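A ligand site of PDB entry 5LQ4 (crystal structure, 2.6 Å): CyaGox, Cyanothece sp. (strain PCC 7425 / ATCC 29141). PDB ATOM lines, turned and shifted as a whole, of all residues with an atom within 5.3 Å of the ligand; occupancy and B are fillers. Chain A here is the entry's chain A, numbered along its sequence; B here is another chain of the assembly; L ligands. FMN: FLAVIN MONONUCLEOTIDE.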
ATOM      1  N   ARG A 276      -3.736   7.776   4.913  1.00  0.00           N
ATOM      2  CA  ARG A 276      -4.052   6.419   4.462  1.00  0.00           C
ATOM      3  C   ARG A 276      -2.981   5.395   4.869  1.00  0.00           C
ATOM      4  O   ARG A 276      -1.799   5.569   4.553  1.00  0.00           O
ATOM      5  CB  ARG A 276      -4.247   6.385   2.942  1.00  0.00           C
ATOM      6  CG  ARG A 276      -4.678   5.050   2.365  1.00  0.00           C
ATOM      7  CD  ARG A 276      -4.100   4.830   0.978  1.00  0.00           C
ATOM      8  NE  ARG A 276      -2.642   4.898   1.014  1.00  0.00           N
ATOM      9  CZ  ARG A 276      -1.841   3.924   1.442  1.00  0.00           C
ATOM     10  NH1 ARG A 276      -2.348   2.771   1.894  1.00  0.00           N
ATOM     11  NH2 ARG A 276      -0.518   4.105   1.421  1.00  0.00           N
ATOM     12  N   ARG A 277      -3.427   4.347   5.548  1.00  0.00           N
ATOM     13  CA  ARG A 277      -2.594   3.207   5.974  1.00  0.00           C
ATOM     14  C   ARG A 277      -3.338   1.917   5.628  1.00  0.00           C
ATOM     15  O   ARG A 277      -4.568   1.900   5.523  1.00  0.00           O
ATOM     16  CB  ARG A 277      -2.321   3.194   7.484  1.00  0.00           C
ATOM     17  CG  ARG A 277      -2.080   4.514   8.195  1.00  0.00           C
ATOM     18  CD  ARG A 277      -1.520   4.240   9.585  1.00  0.00           C
ATOM     19  NE  ARG A 277      -1.685   5.352  10.529  1.00  0.00           N
ATOM     20  CZ  ARG A 277      -0.983   5.517  11.656  1.00  0.00           C
ATOM     21  NH1 ARG A 277      -0.041   4.651  12.020  1.00  0.00           N
ATOM     22  NH2 ARG A 277      -1.244   6.570  12.439  1.00  0.00           N
ATOM     23  N   SER A 278      -2.587   0.832   5.480  1.00  0.00           N
ATOM     24  CA  SER A 278      -3.174  -0.513   5.455  1.00  0.00           C
ATOM     25  C   SER A 278      -3.242  -0.965   6.893  1.00  0.00           C
ATOM     26  O   SER A 278      -2.223  -0.991   7.584  1.00  0.00           O
ATOM     27  CB  SER A 278      -2.321  -1.473   4.636  1.00  0.00           C
ATOM     28  OG  SER A 278      -2.423  -1.187   3.260  1.00  0.00           O
ATOM     29  N   ARG A 280      -4.581  -3.941   9.431  1.00  0.00           N
ATOM     30  CA  ARG A 280      -4.924  -5.352   9.492  1.00  0.00           C
ATOM     31  C   ARG A 280      -5.372  -5.812  10.872  1.00  0.00           C
ATOM     32  O   ARG A 280      -6.012  -6.844  10.970  1.00  0.00           O
ATOM     33  CB  ARG A 280      -3.737  -6.183   9.032  1.00  0.00           C
ATOM     34  CG  ARG A 280      -3.311  -5.889   7.603  1.00  0.00           C
ATOM     35  CD  ARG A 280      -1.864  -6.300   7.368  1.00  0.00           C
ATOM     36  NE  ARG A 280      -1.027  -5.342   6.643  1.00  0.00           N
ATOM     37  CZ  ARG A 280      -1.067  -5.049   5.348  1.00  0.00           C
ATOM     38  NH1 ARG A 280      -1.965  -5.608   4.560  1.00  0.00           N
ATOM     39  NH2 ARG A 280      -0.202  -4.160   4.861  1.00  0.00           N
ATOM     40  N   ALA A 378      -3.238 -14.322   3.788  1.00  0.00           N
ATOM     41  CA  ALA A 378      -2.679 -13.353   2.854  1.00  0.00           C
ATOM     42  C   ALA A 378      -2.357 -11.995   3.483  1.00  0.00           C
ATOM     43  O   ALA A 378      -1.571 -11.234   2.925  1.00  0.00           O
ATOM     44  CB  ALA A 378      -3.622 -13.146   1.680  1.00  0.00           C
ATOM     45  N   THR A 379      -2.996 -11.696   4.610  1.00  0.00           N
ATOM     46  CA  THR A 379      -2.854 -10.427   5.290  1.00  0.00           C
ATOM     47  C   THR A 379      -2.002 -10.592   6.576  1.00  0.00           C
ATOM     48  O   THR A 379      -2.032  -9.762   7.475  1.00  0.00           O
ATOM     49  CB  THR A 379      -4.296  -9.834   5.475  1.00  0.00           C
ATOM     50  OG1 THR A 379      -4.256  -8.408   5.579  1.00  0.00           O
ATOM     51  CG2 THR A 379      -5.045 -10.426   6.649  1.00  0.00           C
ATOM     52  N   GLY A 380      -1.206 -11.666   6.621  1.00  0.00           N
ATOM     53  CA  GLY A 380      -0.213 -11.873   7.675  1.00  0.00           C
ATOM     54  C   GLY A 380      -0.689 -12.545   8.951  1.00  0.00           C
ATOM     55  O   GLY A 380       0.091 -12.675   9.892  1.00  0.00           O
ATOM     56  N   TYR A 418      -9.607  -0.247  -5.525  1.00  0.00           N
ATOM     57  CA  TYR A 418      -8.759  -0.377  -4.316  1.00  0.00           C
ATOM     58  C   TYR A 418      -8.402   0.955  -3.680  1.00  0.00           C
ATOM     59  O   TYR A 418      -8.571   1.132  -2.473  1.00  0.00           O
ATOM     60  CB  TYR A 418      -7.457  -1.111  -4.633  1.00  0.00           C
ATOM     61  CG  TYR A 418      -7.543  -2.605  -4.750  1.00  0.00           C
ATOM     62  CD1 TYR A 418      -8.777  -3.312  -4.719  1.00  0.00           C
ATOM     63  CD2 TYR A 418      -6.383  -3.346  -4.922  1.00  0.00           C
ATOM     64  CE1 TYR A 418      -8.806  -4.691  -4.846  1.00  0.00           C
ATOM     65  CE2 TYR A 418      -6.418  -4.722  -5.033  1.00  0.00           C
ATOM     66  CZ  TYR A 418      -7.621  -5.394  -5.008  1.00  0.00           C
ATOM     67  OH  TYR A 418      -7.611  -6.756  -5.129  1.00  0.00           O
ATOM     68  N   TYR A 422      -9.631   2.480  -0.198  1.00  0.00           N
ATOM     69  CA  TYR A 422      -8.617   2.909   0.781  1.00  0.00           C
ATOM     70  C   TYR A 422      -8.897   4.305   1.349  1.00  0.00           C
ATOM     71  O   TYR A 422      -8.828   4.511   2.565  1.00  0.00           O
ATOM     72  CB  TYR A 422      -7.215   2.900   0.164  1.00  0.00           C
ATOM     73  CG  TYR A 422      -6.361   1.679   0.462  1.00  0.00           C
ATOM     74  CD1 TYR A 422      -5.851   1.459   1.733  1.00  0.00           C
ATOM     75  CD2 TYR A 422      -6.009   0.786  -0.547  1.00  0.00           C
ATOM     76  CE1 TYR A 422      -5.047   0.365   2.006  1.00  0.00           C
ATOM     77  CE2 TYR A 422      -5.207  -0.308  -0.288  1.00  0.00           C
ATOM     78  CZ  TYR A 422      -4.725  -0.512   0.982  1.00  0.00           C
ATOM     79  OH  TYR A 422      -3.917  -1.609   1.225  1.00  0.00           O
ATOM     80  N   SER A 433      -7.376  -3.034   3.820  1.00  0.00           N
ATOM     81  CA  SER A 433      -6.194  -3.578   3.148  1.00  0.00           C
ATOM     82  C   SER A 433      -6.592  -4.299   1.885  1.00  0.00           C
ATOM     83  O   SER A 433      -7.505  -5.123   1.891  1.00  0.00           O
ATOM     84  CB  SER A 433      -5.427  -4.545   4.059  1.00  0.00           C
ATOM     85  OG  SER A 433      -4.166  -4.872   3.474  1.00  0.00           O
ATOM     86  N   ALA A 434      -5.879  -3.981   0.809  1.00  0.00           N
ATOM     87  CA  ALA A 434      -5.955  -4.757  -0.421  1.00  0.00           C
ATOM     88  C   ALA A 434      -5.340  -6.143  -0.191  1.00  0.00           C
ATOM     89  O   ALA A 434      -4.542  -6.332   0.724  1.00  0.00           O
ATOM     90  CB  ALA A 434      -5.234  -4.044  -1.566  1.00  0.00           C
ATOM     91  N   ILE A 435      -5.766  -7.106  -1.010  1.00  0.00           N
ATOM     92  CA  ILE A 435      -5.262  -8.481  -0.959  1.00  0.00           C
ATOM     93  C   ILE A 435      -4.825  -8.851  -2.377  1.00  0.00           C
ATOM     94  O   ILE A 435      -5.569  -8.629  -3.339  1.00  0.00           O
ATOM     95  CB  ILE A 435      -6.322  -9.460  -0.397  1.00  0.00           C
ATOM     96  CG1 ILE A 435      -6.717  -9.036   1.034  1.00  0.00           C
ATOM     97  CG2 ILE A 435      -5.789 -10.883  -0.389  1.00  0.00           C
ATOM     98  CD1 ILE A 435      -7.887  -9.801   1.608  1.00  0.00           C
ATOM     99  N   GLY A 436      -3.619  -9.388  -2.491  1.00  0.00           N
ATOM    100  CA  GLY A 436      -2.975  -9.594  -3.790  1.00  0.00           C
ATOM    101  C   GLY A 436      -3.489 -10.780  -4.580  1.00  0.00           C
ATOM    102  O   GLY A 436      -3.577 -10.714  -5.803  1.00  0.00           O
ATOM    103  N   ALA A 437      -3.843 -11.856  -3.877  1.00  0.00           N
ATOM    104  CA  ALA A 437      -4.217 -13.115  -4.501  1.00  0.00           C
ATOM    105  C   ALA A 437      -5.585 -13.593  -4.035  1.00  0.00           C
ATOM    106  O   ALA A 437      -6.153 -13.072  -3.065  1.00  0.00           O
ATOM    107  CB  ALA A 437      -3.172 -14.164  -4.176  1.00  0.00           C
ATOM    108  N   THR B 322       8.128   4.777   1.608  1.00  0.00           N
ATOM    109  CA  THR B 322       6.696   5.028   1.708  1.00  0.00           C
ATOM    110  C   THR B 322       6.352   6.145   0.688  1.00  0.00           C
ATOM    111  O   THR B 322       7.165   7.048   0.444  1.00  0.00           O
ATOM    112  CB  THR B 322       6.234   5.290   3.172  1.00  0.00           C
ATOM    113  OG1 THR B 322       4.824   5.522   3.202  1.00  0.00           O
ATOM    114  CG2 THR B 322       6.937   6.460   3.814  1.00  0.00           C
ATOM    115  N   PRO B 326      -0.815   3.009  -1.969  1.00  0.00           N
ATOM    116  CA  PRO B 326      -0.475   1.662  -1.523  1.00  0.00           C
ATOM    117  C   PRO B 326       0.184   0.852  -2.631  1.00  0.00           C
ATOM    118  O   PRO B 326       0.007   1.166  -3.797  1.00  0.00           O
ATOM    119  CB  PRO B 326      -1.825   1.054  -1.177  1.00  0.00           C
ATOM    120  CG  PRO B 326      -2.756   1.714  -2.131  1.00  0.00           C
ATOM    121  CD  PRO B 326      -2.266   3.145  -2.185  1.00  0.00           C
ATOM    122  N   SER B 327       0.911  -0.190  -2.247  1.00  0.00           N
ATOM    123  CA  SER B 327       1.637  -1.027  -3.196  1.00  0.00           C
ATOM    124  C   SER B 327       1.967  -2.384  -2.582  1.00  0.00           C
ATOM    125  O   SER B 327       2.622  -2.469  -1.542  1.00  0.00           O
ATOM    126  CB  SER B 327       2.915  -0.328  -3.670  1.00  0.00           C
ATOM    127  OG  SER B 327       3.452  -0.953  -4.823  1.00  0.00           O
ATOM    128  N   GLY B 328       1.381  -3.425  -3.174  1.00  0.00           N
ATOM    129  CA  GLY B 328       1.783  -4.822  -3.015  1.00  0.00           C
ATOM    130  C   GLY B 328       3.237  -5.057  -2.686  1.00  0.00           C
ATOM    131  O   GLY B 328       4.124  -4.749  -3.480  1.00  0.00           O
ATOM    132  N   GLY B 329       3.458  -5.606  -1.503  1.00  0.00           N
ATOM    133  CA  GLY B 329       4.788  -5.904  -0.997  1.00  0.00           C
ATOM    134  C   GLY B 329       5.600  -4.707  -0.594  1.00  0.00           C
ATOM    135  O   GLY B 329       6.779  -4.841  -0.293  1.00  0.00           O
ATOM    136  N   ALA B 330       4.969  -3.530  -0.528  1.00  0.00           N
ATOM    137  CA  ALA B 330       5.673  -2.241  -0.571  1.00  0.00           C
ATOM    138  C   ALA B 330       6.492  -2.242  -1.868  1.00  0.00           C
ATOM    139  O   ALA B 330       5.894  -2.415  -2.952  1.00  0.00           O
ATOM    140  CB  ALA B 330       6.501  -2.005   0.690  1.00  0.00           C
ATOM    141  N   TYR B 332       7.452  -0.723  -4.447  1.00  0.00           N
ATOM    142  CA  TYR B 332       7.269   0.472  -5.282  1.00  0.00           C
ATOM    143  C   TYR B 332       8.130   0.451  -6.552  1.00  0.00           C
ATOM    144  O   TYR B 332       9.093   1.222  -6.700  1.00  0.00           O
ATOM    145  CB  TYR B 332       7.515   1.730  -4.450  1.00  0.00           C
ATOM    146  CG  TYR B 332       6.415   1.990  -3.459  1.00  0.00           C
ATOM    147  CD1 TYR B 332       5.213   2.520  -3.874  1.00  0.00           C
ATOM    148  CD2 TYR B 332       6.566   1.673  -2.108  1.00  0.00           C
ATOM    149  CE1 TYR B 332       4.189   2.751  -2.986  1.00  0.00           C
ATOM    150  CE2 TYR B 332       5.545   1.903  -1.206  1.00  0.00           C
ATOM    151  CZ  TYR B 332       4.359   2.441  -1.653  1.00  0.00           C
ATOM    152  OH  TYR B 332       3.325   2.658  -0.792  1.00  0.00           O
ATOM    153  N   LEU B 411      -0.279  -7.678 -10.077  1.00  0.00           N
ATOM    154  CA  LEU B 411      -0.065  -6.624  -9.082  1.00  0.00           C
ATOM    155  C   LEU B 411       0.303  -5.282  -9.727  1.00  0.00           C
ATOM    156  O   LEU B 411      -0.275  -4.256  -9.384  1.00  0.00           O
ATOM    157  CB  LEU B 411       1.021  -6.997  -8.093  1.00  0.00           C
ATOM    158  CG  LEU B 411       0.631  -7.997  -7.020  1.00  0.00           C
ATOM    159  CD1 LEU B 411       1.896  -8.434  -6.307  1.00  0.00           C
ATOM    160  CD2 LEU B 411      -0.367  -7.384  -6.046  1.00  0.00           C
ATOM    161  N   LYS B 414      -2.686  -3.554 -11.249  1.00  0.00           N
ATOM    162  CA  LYS B 414      -3.485  -2.968 -10.158  1.00  0.00           C
ATOM    163  C   LYS B 414      -2.840  -1.728  -9.540  1.00  0.00           C
ATOM    164  O   LYS B 414      -3.546  -0.814  -9.121  1.00  0.00           O
ATOM    165  CB  LYS B 414      -3.753  -3.975  -9.053  1.00  0.00           C
ATOM    166  CG  LYS B 414      -4.681  -5.092  -9.474  1.00  0.00           C
ATOM    167  CD  LYS B 414      -4.742  -6.138  -8.398  1.00  0.00           C
ATOM    168  CE  LYS B 414      -5.448  -7.360  -8.924  1.00  0.00           C
ATOM    169  NZ  LYS B 414      -5.534  -8.360  -7.835  1.00  0.00           N
ATOM    170  N   HIS B 415      -1.504  -1.711  -9.493  1.00  0.00           N
ATOM    171  CA  HIS B 415      -0.783  -0.499  -9.085  1.00  0.00           C
ATOM    172  C   HIS B 415      -0.985   0.664 -10.061  1.00  0.00           C
ATOM    173  O   HIS B 415      -1.085   1.818  -9.636  1.00  0.00           O
ATOM    174  CB  HIS B 415       0.728  -0.760  -8.898  1.00  0.00           C
ATOM    175  CG  HIS B 415       1.027  -1.795  -7.861  1.00  0.00           C
ATOM    176  ND1 HIS B 415       2.190  -2.535  -7.867  1.00  0.00           N
ATOM    177  CD2 HIS B 415       0.298  -2.243  -6.812  1.00  0.00           C
ATOM    178  CE1 HIS B 415       2.182  -3.377  -6.858  1.00  0.00           C
ATOM    179  NE2 HIS B 415       1.046  -3.212  -6.193  1.00  0.00           N
ATOM    180  N   VAL B 418      -4.343   1.975  -9.193  1.00  0.00           N
ATOM    181  CA  VAL B 418      -4.212   2.692  -7.918  1.00  0.00           C
ATOM    182  C   VAL B 418      -3.664   4.095  -8.159  1.00  0.00           C
ATOM    183  O   VAL B 418      -4.140   5.072  -7.564  1.00  0.00           O
ATOM    184  CB  VAL B 418      -3.310   1.917  -6.924  1.00  0.00           C
ATOM    185  CG1 VAL B 418      -2.817   2.816  -5.788  1.00  0.00           C
ATOM    186  CG2 VAL B 418      -4.053   0.704  -6.373  1.00  0.00           C
HETATM  187  N1  FMN L   1      -1.208  -6.379   1.987  1.00  0.00           N
HETATM  188  C2  FMN L   1      -1.202  -7.654   2.468  1.00  0.00           C
HETATM  189  O2  FMN L   1      -0.995  -7.811   3.686  1.00  0.00           O
HETATM  190  N3  FMN L   1      -1.419  -8.733   1.697  1.00  0.00           N
HETATM  191  C4  FMN L   1      -1.660  -8.622   0.391  1.00  0.00           C
HETATM  192  O4  FMN L   1      -1.862  -9.642  -0.296  1.00  0.00           O
HETATM  193  C4A FMN L   1      -1.683  -7.274  -0.230  1.00  0.00           C
HETATM  194  N5  FMN L   1      -1.911  -7.086  -1.545  1.00  0.00           N
HETATM  195  C5A FMN L   1      -1.922  -5.849  -2.091  1.00  0.00           C
HETATM  196  C6  FMN L   1      -2.187  -5.734  -3.464  1.00  0.00           C
HETATM  197  C7  FMN L   1      -2.212  -4.496  -4.079  1.00  0.00           C
HETATM  198  C7M FMN L   1      -2.496  -4.410  -5.550  1.00  0.00           C
HETATM  199  C8  FMN L   1      -1.977  -3.265  -3.260  1.00  0.00           C
HETATM  200  C8M FMN L   1      -1.995  -1.896  -3.888  1.00  0.00           C
HETATM  201  C9  FMN L   1      -1.715  -3.379  -1.900  1.00  0.00           C
HETATM  202  C9A FMN L   1      -1.689  -4.631  -1.257  1.00  0.00           C
HETATM  203  N10 FMN L   1      -1.441  -4.807   0.127  1.00  0.00           N
HETATM  204  C10 FMN L   1      -1.433  -6.110   0.665  1.00  0.00           C
HETATM  205  C1' FMN L   1      -1.186  -3.659   1.020  1.00  0.00           C
HETATM  206  C2' FMN L   1       0.293  -3.315   0.933  1.00  0.00           C
HETATM  207  O2' FMN L   1       1.047  -4.368   1.557  1.00  0.00           O
HETATM  208  C3' FMN L   1       0.584  -1.976   1.598  1.00  0.00           C
HETATM  209  O3' FMN L   1       0.100  -0.949   0.715  1.00  0.00           O
HETATM  210  C4' FMN L   1       2.072  -1.776   1.926  1.00  0.00           C
HETATM  211  O4' FMN L   1       2.679  -3.018   2.304  1.00  0.00           O
HETATM  212  C5' FMN L   1       2.276  -0.835   3.102  1.00  0.00           C
HETATM  213  O5' FMN L   1       1.823   0.479   2.780  1.00  0.00           O
HETATM  214  P   FMN L   1       0.532   1.170   3.469  1.00  0.00           P
HETATM  215  O1P FMN L   1       0.466   0.695   4.900  1.00  0.00           O
HETATM  216  O2P FMN L   1       0.834   2.641   3.324  1.00  0.00           O
HETATM  217  O3P FMN L   1      -0.648   0.728   2.640  1.00  0.00           O
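The guanidinium group of Arg 280 sits at hydrogen-bond distance from an oxygen (O2) of the ligand, 2.6 Å away.
An oxygen (O3') of the ligand sits at hydrogen-bond distance from the backbone NH (N) of Ser 327 of chain B (3.2 Å).
N of Gly 436 lies within hydrogen-bond range of O4 of the ligand (2.8 Å).
O of Ala 378 lies within hydrogen-bond range of N3 of the ligand (2.8 Å).
An oxygen (O3P) of the ligand lies within hydrogen-bond range of the side-chain hydroxyl (OG) of Ser 278 (2.7 Å).
An oxygen (O1P) of the ligand sits at hydrogen-bond distance from the backbone NH of Ser 278 (3.1 Å).
NH2 of Arg 276 is in salt-bridge range of O2P of the ligand.
The guanidinium group (NH1) of Arg 280 lies within hydrogen-bond range of the side-chain hydroxyl (OG) of Ser 433, at 2.6 Å.
OH of Tyr 422 lies within hydrogen-bond range of N of Ala 434.
OH of Tyr 422 lies within hydrogen-bond range of OG of Ser 278 (2.6 Å).
The side-chain hydroxyl (OH) of Tyr 418 of chain A sits at hydrogen-bond distance from the backbone carbonyl oxygen (O) of Ile 435, 3.3 Å away.
O of Leu 411 of chain B lies close to ND1 of His 415 of chain B (3.4 Å).
The backbone NH (N) of Gly 328 of chain B sits at hydrogen-bond distance from a ring nitrogen (NE2) of His 415 of chain B (3.0 Å).
OG of Ser 327 of chain B is in hydrogen-bond range of O of Ala 330 of chain B (3.4 Å).
Merely in contact with the ligand: Ala 434, Gly 328 of chain B, Pro 326 of chain B, Tyr 422, Ile 435, Leu 411 of chain B, Thr 379, Ser 433, Ala 330 of chain B, His 415 of chain B, Lys 414 of chain B and Tyr 418 of chain A.
Hydrophobic or aromatic side chains within 4 Å of the ligand: Tyr 418 of chain A, Ala 434, Pro 326 of chain B, Leu 411 of chain B and His 415 of chain B.
Within 4 Å of the ligand: Arg 276, Ser 278, Arg 280, Ala 378, Thr 379, Tyr 418 of chain A, Tyr 422, Ser 433, Ala 434, Ile 435, Gly 436, Pro 326 of chain B, Ser 327 of chain B, Gly 328 of chain B, Ala 330 of chain B, Leu 411 of chain B, Lys 414 of chain B and His 415 of chain B.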
